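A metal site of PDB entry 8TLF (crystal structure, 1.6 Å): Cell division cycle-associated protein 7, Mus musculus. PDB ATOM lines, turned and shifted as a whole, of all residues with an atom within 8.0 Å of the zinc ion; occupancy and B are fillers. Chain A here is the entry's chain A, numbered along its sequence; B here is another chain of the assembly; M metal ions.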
ATOM      1  N   CYS A  27      -2.758 -11.286   5.125  1.00  0.00           N
ATOM      2  CA  CYS A  27      -2.535 -12.179   3.996  1.00  0.00           C
ATOM      3  C   CYS A  27      -3.854 -12.752   3.490  1.00  0.00           C
ATOM      4  O   CYS A  27      -4.702 -13.188   4.289  1.00  0.00           O
ATOM      5  CB  CYS A  27      -1.591 -13.313   4.413  1.00  0.00           C
ATOM      6  SG  CYS A  27      -1.283 -14.522   3.113  1.00  0.00           S
ATOM      7  N   SER A  30      -1.739 -17.788   1.011  1.00  0.00           N
ATOM      8  CA  SER A  30      -0.493 -18.153   1.697  1.00  0.00           C
ATOM      9  C   SER A  30       0.700 -18.158   0.750  1.00  0.00           C
ATOM     10  O   SER A  30       1.840 -17.968   1.197  1.00  0.00           O
ATOM     11  CB  SER A  30      -0.653 -19.526   2.354  1.00  0.00           C
ATOM     12  OG  SER A  30      -0.956 -20.518   1.392  1.00  0.00           O
ATOM     13  N   LYS A  33       2.907 -14.737   0.598  1.00  0.00           N
ATOM     14  CA  LYS A  33       3.573 -14.212   1.781  1.00  0.00           C
ATOM     15  C   LYS A  33       4.999 -13.783   1.458  1.00  0.00           C
ATOM     16  O   LYS A  33       5.657 -14.313   0.559  1.00  0.00           O
ATOM     17  CB  LYS A  33       3.599 -15.266   2.892  1.00  0.00           C
ATOM     18  CG  LYS A  33       2.242 -15.599   3.473  1.00  0.00           C
ATOM     19  CD  LYS A  33       2.378 -16.601   4.606  1.00  0.00           C
ATOM     20  CE  LYS A  33       1.052 -16.861   5.293  1.00  0.00           C
ATOM     21  NZ  LYS A  33       1.194 -17.820   6.420  1.00  0.00           N
ATOM     22  N   THR A  42       5.854 -15.008  13.257  1.00  0.00           N
ATOM     23  CA  THR A  42       5.551 -16.414  13.031  1.00  0.00           C
ATOM     24  C   THR A  42       4.083 -16.697  13.328  1.00  0.00           C
ATOM     25  O   THR A  42       3.577 -16.335  14.388  1.00  0.00           O
ATOM     26  CB  THR A  42       6.445 -17.310  13.892  1.00  0.00           C
ATOM     27  OG1 THR A  42       7.819 -17.066  13.564  1.00  0.00           O
ATOM     28  CG2 THR A  42       6.124 -18.776  13.651  1.00  0.00           C
ATOM     29  N   CYS A  43       3.414 -17.348  12.375  1.00  0.00           N
ATOM     30  CA  CYS A  43       2.065 -17.847  12.600  1.00  0.00           C
ATOM     31  C   CYS A  43       2.139 -19.173  13.345  1.00  0.00           C
ATOM     32  O   CYS A  43       2.888 -20.064  12.965  1.00  0.00           O
ATOM     33  CB  CYS A  43       1.328 -18.024  11.269  1.00  0.00           C
ATOM     34  SG  CYS A  43      -0.216 -18.948  11.381  1.00  0.00           S
ATOM     35  N   HIS A  44       1.353 -19.297  14.420  1.00  0.00           N
ATOM     36  CA  HIS A  44       1.396 -20.515  15.226  1.00  0.00           C
ATOM     37  C   HIS A  44       0.942 -21.732  14.418  1.00  0.00           C
ATOM     38  O   HIS A  44       1.466 -22.836  14.628  1.00  0.00           O
ATOM     39  CB  HIS A  44       0.519 -20.365  16.468  1.00  0.00           C
ATOM     40  CG  HIS A  44       0.361 -21.627  17.255  1.00  0.00           C
ATOM     41  ND1 HIS A  44       1.379 -22.174  17.993  1.00  0.00           N
ATOM     42  CD2 HIS A  44      -0.700 -22.454  17.393  1.00  0.00           C
ATOM     43  CE1 HIS A  44       0.949 -23.287  18.569  1.00  0.00           C
ATOM     44  NE2 HIS A  44      -0.302 -23.482  18.225  1.00  0.00           N
ATOM     45  N   GLN A  45      -0.014 -21.554  13.506  1.00  0.00           N
ATOM     46  CA  GLN A  45      -0.588 -22.694  12.799  1.00  0.00           C
ATOM     47  C   GLN A  45       0.381 -23.259  11.769  1.00  0.00           C
ATOM     48  O   GLN A  45       0.712 -24.446  11.796  1.00  0.00           O
ATOM     49  CB  GLN A  45      -1.910 -22.276  12.140  1.00  0.00           C
ATOM     50  CG  GLN A  45      -2.718 -23.439  11.578  1.00  0.00           C
ATOM     51  CD  GLN A  45      -3.516 -24.165  12.641  1.00  0.00           C
ATOM     52  OE1 GLN A  45      -3.784 -23.619  13.710  1.00  0.00           O
ATOM     53  NE2 GLN A  45      -3.901 -25.400  12.352  1.00  0.00           N
ATOM     54  N   CYS A  46       0.823 -22.420  10.826  1.00  0.00           N
ATOM     55  CA  CYS A  46       1.686 -22.868   9.739  1.00  0.00           C
ATOM     56  C   CYS A  46       3.165 -22.715  10.033  1.00  0.00           C
ATOM     57  O   CYS A  46       3.991 -23.211   9.253  1.00  0.00           O
ATOM     58  CB  CYS A  46       1.342 -22.099   8.450  1.00  0.00           C
ATOM     59  SG  CYS A  46       1.586 -20.314   8.550  1.00  0.00           S
ATOM     60  N   ARG A  47       3.535 -22.047  11.125  1.00  0.00           N
ATOM     61  CA  ARG A  47       4.915 -21.919  11.581  1.00  0.00           C
ATOM     62  C   ARG A  47       5.815 -21.235  10.541  1.00  0.00           C
ATOM     63  O   ARG A  47       7.011 -21.526  10.442  1.00  0.00           O
ATOM     64  CB  ARG A  47       5.498 -23.286  11.977  1.00  0.00           C
ATOM     65  CG  ARG A  47       4.661 -23.992  13.052  1.00  0.00           C
ATOM     66  CD  ARG A  47       5.332 -25.248  13.586  1.00  0.00           C
ATOM     67  NE  ARG A  47       5.216 -26.383  12.676  1.00  0.00           N
ATOM     68  CZ  ARG A  47       4.190 -27.217  12.641  1.00  0.00           C
ATOM     69  NH1 ARG A  47       3.146 -27.052  13.438  1.00  0.00           N
ATOM     70  NH2 ARG A  47       4.202 -28.241  11.788  1.00  0.00           N
ATOM     71  N   GLN A  48       5.247 -20.300   9.786  1.00  0.00           N
ATOM     72  CA  GLN A  48       5.989 -19.502   8.821  1.00  0.00           C
ATOM     73  C   GLN A  48       6.156 -18.093   9.362  1.00  0.00           C
ATOM     74  O   GLN A  48       5.191 -17.491   9.843  1.00  0.00           O
ATOM     75  CB  GLN A  48       5.286 -19.465   7.458  1.00  0.00           C
ATOM     76  CG  GLN A  48       4.934 -20.820   6.896  1.00  0.00           C
ATOM     77  CD  GLN A  48       6.152 -21.686   6.656  1.00  0.00           C
ATOM     78  OE1 GLN A  48       6.943 -21.440   5.742  1.00  0.00           O
ATOM     79  NE2 GLN A  48       6.328 -22.712   7.485  1.00  0.00           N
ATOM     80  N   THR A  50       6.620 -14.454   8.524  1.00  0.00           N
ATOM     81  CA  THR A  50       6.406 -13.583   7.391  1.00  0.00           C
ATOM     82  C   THR A  50       5.932 -12.222   7.886  1.00  0.00           C
ATOM     83  O   THR A  50       5.610 -12.036   9.056  1.00  0.00           O
ATOM     84  CB  THR A  50       5.393 -14.181   6.403  1.00  0.00           C
ATOM     85  OG1 THR A  50       4.165 -14.458   7.095  1.00  0.00           O
ATOM     86  CG2 THR A  50       5.923 -15.478   5.802  1.00  0.00           C
ATOM     87  N   ASP A  52       3.235 -10.433   6.902  1.00  0.00           N
ATOM     88  CA  ASP A  52       1.818 -10.101   6.880  1.00  0.00           C
ATOM     89  C   ASP A  52       1.279  -9.949   8.294  1.00  0.00           C
ATOM     90  O   ASP A  52       1.813 -10.486   9.267  1.00  0.00           O
ATOM     91  CB  ASP A  52       1.012 -11.155   6.117  1.00  0.00           C
ATOM     92  CG  ASP A  52       1.421 -12.569   6.474  1.00  0.00           C
ATOM     93  OD1 ASP A  52       2.565 -12.950   6.167  1.00  0.00           O
ATOM     94  OD2 ASP A  52       0.595 -13.301   7.065  1.00  0.00           O
ATOM     95  N   LYS A  54      -0.829 -10.397  11.577  1.00  0.00           N
ATOM     96  CA  LYS A  54      -1.323 -11.580  12.260  1.00  0.00           C
ATOM     97  C   LYS A  54      -2.090 -11.154  13.514  1.00  0.00           C
ATOM     98  O   LYS A  54      -2.014 -10.009  13.954  1.00  0.00           O
ATOM     99  CB  LYS A  54      -0.173 -12.535  12.616  1.00  0.00           C
ATOM    100  CG  LYS A  54       0.598 -12.985  11.390  1.00  0.00           C
ATOM    101  CD  LYS A  54       1.629 -14.048  11.721  1.00  0.00           C
ATOM    102  CE  LYS A  54       2.328 -14.497  10.457  1.00  0.00           C
ATOM    103  NZ  LYS A  54       3.072 -13.374   9.812  1.00  0.00           N
ATOM    104  N   GLN A  68      -0.503 -15.814  17.670  1.00  0.00           N
ATOM    105  CA  GLN A  68      -0.330 -15.167  16.376  1.00  0.00           C
ATOM    106  C   GLN A  68      -0.739 -16.121  15.269  1.00  0.00           C
ATOM    107  O   GLN A  68      -0.153 -17.191  15.109  1.00  0.00           O
ATOM    108  CB  GLN A  68       1.125 -14.732  16.193  1.00  0.00           C
ATOM    109  CG  GLN A  68       1.639 -13.784  17.257  1.00  0.00           C
ATOM    110  CD  GLN A  68       3.100 -13.446  17.095  1.00  0.00           C
ATOM    111  OE1 GLN A  68       3.770 -13.941  16.180  1.00  0.00           O
ATOM    112  NE2 GLN A  68       3.625 -12.607  17.978  1.00  0.00           N
ATOM    113  N   PHE A  69      -1.753 -15.715  14.489  1.00  0.00           N
ATOM    114  CA  PHE A  69      -2.258 -16.501  13.370  1.00  0.00           C
ATOM    115  C   PHE A  69      -2.361 -15.626  12.134  1.00  0.00           C
ATOM    116  O   PHE A  69      -2.794 -14.474  12.207  1.00  0.00           O
ATOM    117  CB  PHE A  69      -3.627 -17.113  13.695  1.00  0.00           C
ATOM    118  CG  PHE A  69      -3.566 -18.228  14.700  1.00  0.00           C
ATOM    119  CD1 PHE A  69      -3.467 -17.969  16.056  1.00  0.00           C
ATOM    120  CD2 PHE A  69      -3.613 -19.553  14.284  1.00  0.00           C
ATOM    121  CE1 PHE A  69      -3.417 -18.997  16.978  1.00  0.00           C
ATOM    122  CE2 PHE A  69      -3.571 -20.586  15.206  1.00  0.00           C
ATOM    123  CZ  PHE A  69      -3.462 -20.305  16.543  1.00  0.00           C
ATOM    124  N   CYS A  70      -1.977 -16.191  10.989  1.00  0.00           N
ATOM    125  CA  CYS A  70      -2.070 -15.467   9.730  1.00  0.00           C
ATOM    126  C   CYS A  70      -3.497 -15.508   9.193  1.00  0.00           C
ATOM    127  O   CYS A  70      -4.376 -16.198   9.729  1.00  0.00           O
ATOM    128  CB  CYS A  70      -1.087 -16.035   8.709  1.00  0.00           C
ATOM    129  SG  CYS A  70      -1.496 -17.685   8.093  1.00  0.00           S
ATOM    130  N   GLY A  71      -3.723 -14.762   8.110  1.00  0.00           N
ATOM    131  CA  GLY A  71      -5.026 -14.681   7.490  1.00  0.00           C
ATOM    132  C   GLY A  71      -5.578 -16.018   7.037  1.00  0.00           C
ATOM    133  O   GLY A  71      -6.635 -16.455   7.489  1.00  0.00           O
ATOM    134  N   PRO A  72      -4.887 -16.681   6.096  1.00  0.00           N
ATOM    135  CA  PRO A  72      -5.404 -17.963   5.596  1.00  0.00           C
ATOM    136  C   PRO A  72      -5.587 -19.014   6.673  1.00  0.00           C
ATOM    137  O   PRO A  72      -6.578 -19.761   6.645  1.00  0.00           O
ATOM    138  CB  PRO A  72      -4.340 -18.385   4.565  1.00  0.00           C
ATOM    139  CG  PRO A  72      -3.718 -17.100   4.129  1.00  0.00           C
ATOM    140  CD  PRO A  72      -3.697 -16.227   5.350  1.00  0.00           C
ATOM    141  N   CYS A  73      -4.666 -19.111   7.633  1.00  0.00           N
ATOM    142  CA  CYS A  73      -4.777 -20.142   8.661  1.00  0.00           C
ATOM    143  C   CYS A  73      -5.976 -19.903   9.568  1.00  0.00           C
ATOM    144  O   CYS A  73      -6.683 -20.859   9.936  1.00  0.00           O
ATOM    145  CB  CYS A  73      -3.494 -20.223   9.482  1.00  0.00           C
ATOM    146  SG  CYS A  73      -2.153 -21.110   8.654  1.00  0.00           S
ATOM    147  N   LEU A  74      -6.230 -18.655   9.946  1.00  0.00           N
ATOM    148  CA  LEU A  74      -7.359 -18.375  10.825  1.00  0.00           C
ATOM    149  C   LEU A  74      -8.692 -18.679  10.143  1.00  0.00           C
ATOM    150  O   LEU A  74      -9.598 -19.249  10.770  1.00  0.00           O
ATOM    151  CB  LEU A  74      -7.319 -16.924  11.293  1.00  0.00           C
ATOM    152  CG  LEU A  74      -8.267 -16.619  12.451  1.00  0.00           C
ATOM    153  CD1 LEU A  74      -7.860 -17.387  13.698  1.00  0.00           C
ATOM    154  CD2 LEU A  74      -8.327 -15.122  12.735  1.00  0.00           C
ATOM    155  N   ARG A  77      -8.766 -22.758   9.184  1.00  0.00           N
ATOM    156  CA  ARG A  77      -8.747 -23.716  10.284  1.00  0.00           C
ATOM    157  C   ARG A  77      -9.762 -23.401  11.374  1.00  0.00           C
ATOM    158  O   ARG A  77     -10.082 -24.298  12.168  1.00  0.00           O
ATOM    159  CB  ARG A  77      -7.347 -23.778  10.903  1.00  0.00           C
ATOM    160  CG  ARG A  77      -6.223 -24.011   9.907  1.00  0.00           C
ATOM    161  CD  ARG A  77      -6.295 -25.392   9.275  1.00  0.00           C
ATOM    162  NE  ARG A  77      -6.103 -26.449  10.262  1.00  0.00           N
ATOM    163  CZ  ARG A  77      -5.827 -27.713   9.952  1.00  0.00           C
ATOM    164  NH1 ARG A  77      -5.700 -28.105   8.699  1.00  0.00           N
ATOM    165  NH2 ARG A  77      -5.672 -28.598  10.935  1.00  0.00           N
ATOM    166  P    DT B  13      -4.634 -25.746   5.623  1.00  0.00           P
ATOM    167  OP1  DT B  13      -5.742 -26.498   6.251  1.00  0.00           O
ATOM    168  OP2  DT B  13      -4.333 -24.366   6.068  1.00  0.00           O
ATOM    169  O5'  DT B  13      -3.285 -26.607   5.751  1.00  0.00           O
ATOM    170  C5'  DT B  13      -3.280 -27.970   5.350  1.00  0.00           C
ATOM    171  C4'  DT B  13      -1.885 -28.552   5.492  1.00  0.00           C
ATOM    172  O4'  DT B  13      -0.984 -27.826   4.647  1.00  0.00           O
ATOM    173  C3'  DT B  13      -1.285 -28.443   6.880  1.00  0.00           C
ATOM    174  O3'  DT B  13      -1.679 -29.565   7.656  1.00  0.00           O
ATOM    175  C2'  DT B  13       0.207 -28.453   6.607  1.00  0.00           C
ATOM    176  C1'  DT B  13       0.312 -27.843   5.202  1.00  0.00           C
ATOM    177  N1   DT B  13       0.874 -26.460   5.177  1.00  0.00           N
ATOM    178  C2   DT B  13       2.237 -26.288   5.225  1.00  0.00           C
ATOM    179  O2   DT B  13       3.021 -27.216   5.293  1.00  0.00           O
ATOM    180  N3   DT B  13       2.649 -24.987   5.187  1.00  0.00           N
ATOM    181  C4   DT B  13       1.855 -23.857   5.118  1.00  0.00           C
ATOM    182  O4   DT B  13       2.325 -22.724   5.094  1.00  0.00           O
ATOM    183  C5   DT B  13       0.436 -24.106   5.075  1.00  0.00           C
ATOM    184  C7   DT B  13      -0.528 -22.960   4.991  1.00  0.00           C
ATOM    185  C6   DT B  13       0.015 -25.376   5.106  1.00  0.00           C
HETATM  186 ZN    ZN M   1      -0.517 -19.552   9.127  1.00  0.00          ZN
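SG of Cys 73 is bound to the zinc ion (2.3 Å).
The zinc ion is bound by SG of Cys 46, 2.3 Å away.
The zinc ion is bound by SG of Cys 70 (2.3 Å).
SG of Cys 43 is bound to the zinc ion.
The side-chain amino group (NZ) of Lys 33 sits close to the side-chain sulfur (SG) of Cys 46 (3.3 Å).
NE2 of Gln 48 is in hydrogen-bond range of O of Cys 46 (3.0 Å).
SG of Cys 70 sits close to NZ of Lys 33, 3.2 Å away.
The backbone NH (N) of Gln 45 lies close to the side-chain sulfur (SG) of Cys 43.
O of Gln 48 sits at hydrogen-bond distance from N of Cys 43 (3.1 Å).
Residues that only touch the zinc ion: Lys 33 (3.6 Å).
Within 4 Å of the zinc ion: Lys 33, Cys 43, Cys 46, Cys 70 and Cys 73.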
